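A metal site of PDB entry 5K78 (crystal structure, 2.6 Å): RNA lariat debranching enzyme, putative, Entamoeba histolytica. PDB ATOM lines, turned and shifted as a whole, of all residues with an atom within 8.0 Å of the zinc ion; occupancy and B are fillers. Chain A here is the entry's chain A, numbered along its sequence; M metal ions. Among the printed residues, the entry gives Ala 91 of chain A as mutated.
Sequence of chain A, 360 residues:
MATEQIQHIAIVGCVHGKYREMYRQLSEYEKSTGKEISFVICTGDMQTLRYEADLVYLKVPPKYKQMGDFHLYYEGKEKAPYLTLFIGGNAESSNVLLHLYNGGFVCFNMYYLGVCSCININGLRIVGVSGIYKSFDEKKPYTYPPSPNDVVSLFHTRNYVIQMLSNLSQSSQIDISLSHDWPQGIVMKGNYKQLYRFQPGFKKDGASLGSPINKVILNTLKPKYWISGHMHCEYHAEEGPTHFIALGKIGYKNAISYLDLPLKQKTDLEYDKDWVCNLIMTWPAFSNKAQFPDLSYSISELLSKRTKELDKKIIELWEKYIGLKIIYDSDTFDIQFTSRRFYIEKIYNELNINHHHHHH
The backbone NH (N) of His 16 sits at hydrogen-bond distance from the backbone carbonyl oxygen (O) of Asp 45, at 2.7 Å.
A ring nitrogen (ND1) of His 16 sits at hydrogen-bond distance from the side-chain amide nitrogen (NE2) of Gln 47.
SG of Cys 14 lies close to N of His 230, 3.3 Å away.
The backbone carbonyl oxygen of Gly 248 sits at hydrogen-bond distance from the backbone NH of Cys 14 (3.0 Å).
N of Ile 250 sits at hydrogen-bond distance from O of Cys 14 (2.7 Å).
OD1 of Asp 45 is in hydrogen-bond range of N of Ala 91, 3.1 Å away.
O of His 230 touches the zinc ion, at 3.96 Å.
Within 4 Å of the zinc ion: Cys 14, His 16, Asp 45, His 230 and His 232.
The zinc ion is bound by NE2 of His 232, NE2 of His 16 and SG of Cys 14.
The zinc ion has three donor atoms within binding distance.
Slightly farther from the zinc ion lies OD2 of Asp 45 (2.7 Å).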
ATOM      1  N   GLY A  13      -4.107 -19.130  25.482  1.00  0.00           N
ATOM      2  CA  GLY A  13      -4.443 -17.876  26.131  1.00  0.00           C
ATOM      3  C   GLY A  13      -5.363 -18.058  27.324  1.00  0.00           C
ATOM      4  O   GLY A  13      -5.059 -18.821  28.237  1.00  0.00           O
ATOM      5  N   CYS A  14      -6.481 -17.345  27.326  1.00  0.00           N
ATOM      6  CA  CYS A  14      -7.441 -17.450  28.418  1.00  0.00           C
ATOM      7  C   CYS A  14      -8.290 -18.692  28.245  1.00  0.00           C
ATOM      8  O   CYS A  14      -8.820 -18.943  27.157  1.00  0.00           O
ATOM      9  CB  CYS A  14      -8.331 -16.203  28.473  1.00  0.00           C
ATOM     10  SG  CYS A  14      -7.449 -14.633  28.636  1.00  0.00           S
ATOM     11  N   VAL A  15      -8.441 -19.457  29.327  1.00  0.00           N
ATOM     12  CA  VAL A  15      -9.259 -20.665  29.324  1.00  0.00           C
ATOM     13  C   VAL A  15     -10.669 -20.385  29.833  1.00  0.00           C
ATOM     14  O   VAL A  15     -11.645 -20.827  29.234  1.00  0.00           O
ATOM     15  CB  VAL A  15      -8.580 -21.769  30.163  1.00  0.00           C
ATOM     16  CG1 VAL A  15      -9.479 -23.001  30.257  1.00  0.00           C
ATOM     17  CG2 VAL A  15      -7.224 -22.135  29.564  1.00  0.00           C
ATOM     18  N   HIS A  16     -10.780 -19.635  30.935  1.00  0.00           N
ATOM     19  CA  HIS A  16     -12.067 -19.242  31.506  1.00  0.00           C
ATOM     20  C   HIS A  16     -12.952 -20.462  31.781  1.00  0.00           C
ATOM     21  O   HIS A  16     -14.157 -20.455  31.510  1.00  0.00           O
ATOM     22  CB  HIS A  16     -12.792 -18.239  30.614  1.00  0.00           C
ATOM     23  CG  HIS A  16     -12.238 -16.853  30.681  1.00  0.00           C
ATOM     24  ND1 HIS A  16     -12.434 -16.016  31.765  1.00  0.00           N
ATOM     25  CD2 HIS A  16     -11.485 -16.141  29.800  1.00  0.00           C
ATOM     26  CE1 HIS A  16     -11.835 -14.868  31.549  1.00  0.00           C
ATOM     27  NE2 HIS A  16     -11.241 -14.914  30.366  1.00  0.00           N
ATOM     28  N   THR A  43      -1.899 -18.972  29.889  1.00  0.00           N
ATOM     29  CA  THR A  43      -1.519 -17.633  30.320  1.00  0.00           C
ATOM     30  C   THR A  43      -2.447 -17.055  31.391  1.00  0.00           C
ATOM     31  O   THR A  43      -2.395 -15.848  31.640  1.00  0.00           O
ATOM     32  CB  THR A  43      -1.483 -16.683  29.120  1.00  0.00           C
ATOM     33  OG1 THR A  43      -2.790 -16.585  28.540  1.00  0.00           O
ATOM     34  CG2 THR A  43      -0.500 -17.195  28.078  1.00  0.00           C
ATOM     35  N   GLY A  44      -3.282 -17.873  32.017  1.00  0.00           N
ATOM     36  CA  GLY A  44      -4.078 -17.441  33.145  1.00  0.00           C
ATOM     37  C   GLY A  44      -5.560 -17.486  32.847  1.00  0.00           C
ATOM     38  O   GLY A  44      -6.009 -17.938  31.793  1.00  0.00           O
ATOM     39  N   ASP A  45      -6.340 -16.982  33.817  1.00  0.00           N
ATOM     40  CA  ASP A  45      -7.798 -17.059  33.795  1.00  0.00           C
ATOM     41  C   ASP A  45      -8.260 -18.513  33.685  1.00  0.00           C
ATOM     42  O   ASP A  45      -8.980 -18.901  32.760  1.00  0.00           O
ATOM     43  CB  ASP A  45      -8.391 -16.187  32.691  1.00  0.00           C
ATOM     44  CG  ASP A  45      -8.422 -14.719  33.050  1.00  0.00           C
ATOM     45  OD1 ASP A  45      -7.740 -14.339  34.034  1.00  0.00           O
ATOM     46  OD2 ASP A  45      -9.115 -13.942  32.361  1.00  0.00           O
ATOM     47  N   MET A  46      -7.826 -19.322  34.660  1.00  0.00           N
ATOM     48  CA  MET A  46      -8.087 -20.757  34.633  1.00  0.00           C
ATOM     49  C   MET A  46      -9.366 -21.137  35.360  1.00  0.00           C
ATOM     50  O   MET A  46     -10.003 -22.132  34.976  1.00  0.00           O
ATOM     51  CB  MET A  46      -6.904 -21.499  35.274  1.00  0.00           C
ATOM     52  CG  MET A  46      -5.547 -21.105  34.729  1.00  0.00           C
ATOM     53  SD  MET A  46      -5.303 -21.585  33.010  1.00  0.00           S
ATOM     54  CE  MET A  46      -5.509 -23.361  33.110  1.00  0.00           C
ATOM     55  N   GLN A  47      -9.767 -20.367  36.368  1.00  0.00           N
ATOM     56  CA  GLN A  47     -10.989 -20.620  37.132  1.00  0.00           C
ATOM     57  C   GLN A  47     -11.002 -22.043  37.687  1.00  0.00           C
ATOM     58  O   GLN A  47     -11.905 -22.842  37.428  1.00  0.00           O
ATOM     59  CB  GLN A  47     -12.235 -20.334  36.286  1.00  0.00           C
ATOM     60  CG  GLN A  47     -12.220 -18.978  35.604  1.00  0.00           C
ATOM     61  CD  GLN A  47     -13.556 -18.621  34.997  1.00  0.00           C
ATOM     62  OE1 GLN A  47     -14.513 -19.404  35.063  1.00  0.00           O
ATOM     63  NE2 GLN A  47     -13.636 -17.439  34.391  1.00  0.00           N
ATOM     64  N   GLY A  89      -4.415 -15.561  36.372  1.00  0.00           N
ATOM     65  CA  GLY A  89      -4.860 -14.316  35.773  1.00  0.00           C
ATOM     66  C   GLY A  89      -5.655 -13.466  36.747  1.00  0.00           C
ATOM     67  O   GLY A  89      -5.257 -13.297  37.899  1.00  0.00           O
ATOM     68  N   ASN A  90      -6.790 -12.923  36.281  1.00  0.00           N
ATOM     69  CA  ASN A  90      -7.692 -12.171  37.136  1.00  0.00           C
ATOM     70  C   ASN A  90      -8.984 -12.903  37.448  1.00  0.00           C
ATOM     71  O   ASN A  90      -9.611 -12.606  38.474  1.00  0.00           O
ATOM     72  CB  ASN A  90      -8.024 -10.811  36.508  1.00  0.00           C
ATOM     73  CG  ASN A  90      -8.609 -10.950  35.118  1.00  0.00           C
ATOM     74  OD1 ASN A  90      -7.884 -10.993  34.124  1.00  0.00           O
ATOM     75  ND2 ASN A  90      -9.934 -11.014  35.031  1.00  0.00           N
ATOM     76  N   ALA A  91      -9.400 -13.836  36.589  1.00  0.00           N
ATOM     77  CA  ALA A  91     -10.569 -14.672  36.840  1.00  0.00           C
ATOM     78  C   ALA A  91     -10.043 -16.018  37.342  1.00  0.00           C
ATOM     79  O   ALA A  91      -9.824 -16.951  36.567  1.00  0.00           O
ATOM     80  CB  ALA A  91     -11.416 -14.822  35.583  1.00  0.00           C
ATOM     81  N   HIS A 180       0.166 -12.625  32.390  1.00  0.00           N
ATOM     82  CA  HIS A 180      -1.241 -12.583  31.974  1.00  0.00           C
ATOM     83  C   HIS A 180      -1.487 -11.319  31.160  1.00  0.00           C
ATOM     84  O   HIS A 180      -1.707 -11.389  29.942  1.00  0.00           O
ATOM     85  CB  HIS A 180      -2.172 -12.661  33.191  1.00  0.00           C
ATOM     86  CG  HIS A 180      -3.595 -12.913  32.828  1.00  0.00           C
ATOM     87  ND1 HIS A 180      -3.999 -14.042  32.145  1.00  0.00           N
ATOM     88  CD2 HIS A 180      -4.717 -12.185  33.042  1.00  0.00           C
ATOM     89  CE1 HIS A 180      -5.305 -13.998  31.950  1.00  0.00           C
ATOM     90  NE2 HIS A 180      -5.770 -12.876  32.487  1.00  0.00           N
ATOM     91  N   GLY A 229      -1.819 -13.145  27.654  1.00  0.00           N
ATOM     92  CA  GLY A 229      -3.199 -13.221  27.241  1.00  0.00           C
ATOM     93  C   GLY A 229      -4.034 -12.050  27.696  1.00  0.00           C
ATOM     94  O   GLY A 229      -3.724 -10.899  27.349  1.00  0.00           O
ATOM     95  N   HIS A 230      -5.106 -12.322  28.445  1.00  0.00           N
ATOM     96  CA  HIS A 230      -5.904 -11.305  29.115  1.00  0.00           C
ATOM     97  C   HIS A 230      -6.721 -10.448  28.143  1.00  0.00           C
ATOM     98  O   HIS A 230      -7.874 -10.112  28.437  1.00  0.00           O
ATOM     99  CB  HIS A 230      -5.022 -10.418  30.003  1.00  0.00           C
ATOM    100  CG  HIS A 230      -5.780  -9.395  30.803  1.00  0.00           C
ATOM    101  ND1 HIS A 230      -6.863  -9.723  31.588  1.00  0.00           N
ATOM    102  CD2 HIS A 230      -5.595  -8.070  30.951  1.00  0.00           C
ATOM    103  CE1 HIS A 230      -7.323  -8.635  32.175  1.00  0.00           C
ATOM    104  NE2 HIS A 230      -6.561  -7.611  31.810  1.00  0.00           N
ATOM    105  N   MET A 231      -6.140 -10.106  26.997  1.00  0.00           N
ATOM    106  CA  MET A 231      -6.763  -9.156  26.079  1.00  0.00           C
ATOM    107  C   MET A 231      -7.724  -9.802  25.080  1.00  0.00           C
ATOM    108  O   MET A 231      -8.365  -9.073  24.324  1.00  0.00           O
ATOM    109  CB  MET A 231      -5.685  -8.403  25.306  1.00  0.00           C
ATOM    110  CG  MET A 231      -4.697  -7.657  26.192  1.00  0.00           C
ATOM    111  SD  MET A 231      -5.489  -6.530  27.358  1.00  0.00           S
ATOM    112  CE  MET A 231      -5.806  -5.132  26.285  1.00  0.00           C
ATOM    113  N   HIS A 232      -7.835 -11.132  25.063  1.00  0.00           N
ATOM    114  CA  HIS A 232      -8.800 -11.836  24.216  1.00  0.00           C
ATOM    115  C   HIS A 232      -8.574 -11.528  22.738  1.00  0.00           C
ATOM    116  O   HIS A 232      -9.524 -11.404  21.961  1.00  0.00           O
ATOM    117  CB  HIS A 232     -10.240 -11.517  24.617  1.00  0.00           C
ATOM    118  CG  HIS A 232     -10.595 -11.934  26.004  1.00  0.00           C
ATOM    119  ND1 HIS A 232     -11.696 -11.431  26.678  1.00  0.00           N
ATOM    120  CD2 HIS A 232     -10.013 -12.811  26.862  1.00  0.00           C
ATOM    121  CE1 HIS A 232     -11.775 -11.976  27.871  1.00  0.00           C
ATOM    122  NE2 HIS A 232     -10.760 -12.812  28.006  1.00  0.00           N
ATOM    123  N   LEU A 247      -2.387 -14.153  22.991  1.00  0.00           N
ATOM    124  CA  LEU A 247      -3.356 -15.160  22.601  1.00  0.00           C
ATOM    125  C   LEU A 247      -4.728 -14.711  23.064  1.00  0.00           C
ATOM    126  O   LEU A 247      -4.870 -13.859  23.939  1.00  0.00           O
ATOM    127  CB  LEU A 247      -2.988 -16.536  23.174  1.00  0.00           C
ATOM    128  CG  LEU A 247      -1.575 -17.008  22.837  1.00  0.00           C
ATOM    129  CD1 LEU A 247      -1.198 -18.218  23.668  1.00  0.00           C
ATOM    130  CD2 LEU A 247      -1.438 -17.313  21.344  1.00  0.00           C
ATOM    131  N   GLY A 248      -5.750 -15.301  22.458  1.00  0.00           N
ATOM    132  CA  GLY A 248      -7.123 -14.950  22.729  1.00  0.00           C
ATOM    133  C   GLY A 248      -7.748 -15.879  23.741  1.00  0.00           C
ATOM    134  O   GLY A 248      -7.068 -16.612  24.471  1.00  0.00           O
ATOM    135  N   LYS A 249      -9.067 -15.852  23.790  1.00  0.00           N
ATOM    136  CA  LYS A 249      -9.816 -16.638  24.750  1.00  0.00           C
ATOM    137  C   LYS A 249     -10.310 -17.924  24.106  1.00  0.00           C
ATOM    138  O   LYS A 249     -10.628 -17.957  22.913  1.00  0.00           O
ATOM    139  CB  LYS A 249     -11.009 -15.863  25.299  1.00  0.00           C
ATOM    140  CG  LYS A 249     -11.923 -15.303  24.214  1.00  0.00           C
ATOM    141  CD  LYS A 249     -13.155 -14.660  24.821  1.00  0.00           C
ATOM    142  CE  LYS A 249     -13.929 -15.697  25.627  1.00  0.00           C
ATOM    143  NZ  LYS A 249     -15.071 -15.103  26.364  1.00  0.00           N
ATOM    144  N   ILE A 250     -10.347 -18.999  24.896  1.00  0.00           N
ATOM    145  CA  ILE A 250     -10.871 -20.266  24.406  1.00  0.00           C
ATOM    146  C   ILE A 250     -12.315 -20.085  23.959  1.00  0.00           C
ATOM    147  O   ILE A 250     -13.118 -19.425  24.629  1.00  0.00           O
ATOM    148  CB  ILE A 250     -10.737 -21.350  25.503  1.00  0.00           C
ATOM    149  CG1 ILE A 250      -9.265 -21.706  25.706  1.00  0.00           C
ATOM    150  CG2 ILE A 250     -11.549 -22.574  25.152  1.00  0.00           C
ATOM    151  CD1 ILE A 250      -8.642 -22.404  24.512  1.00  0.00           C
HETATM  152 ZN    ZN M   1      -9.512 -13.469  29.756  1.00  0.00          ZN
HETATM  153 FE    FE M   2      -7.770 -11.875  32.061  1.00  0.00          FE
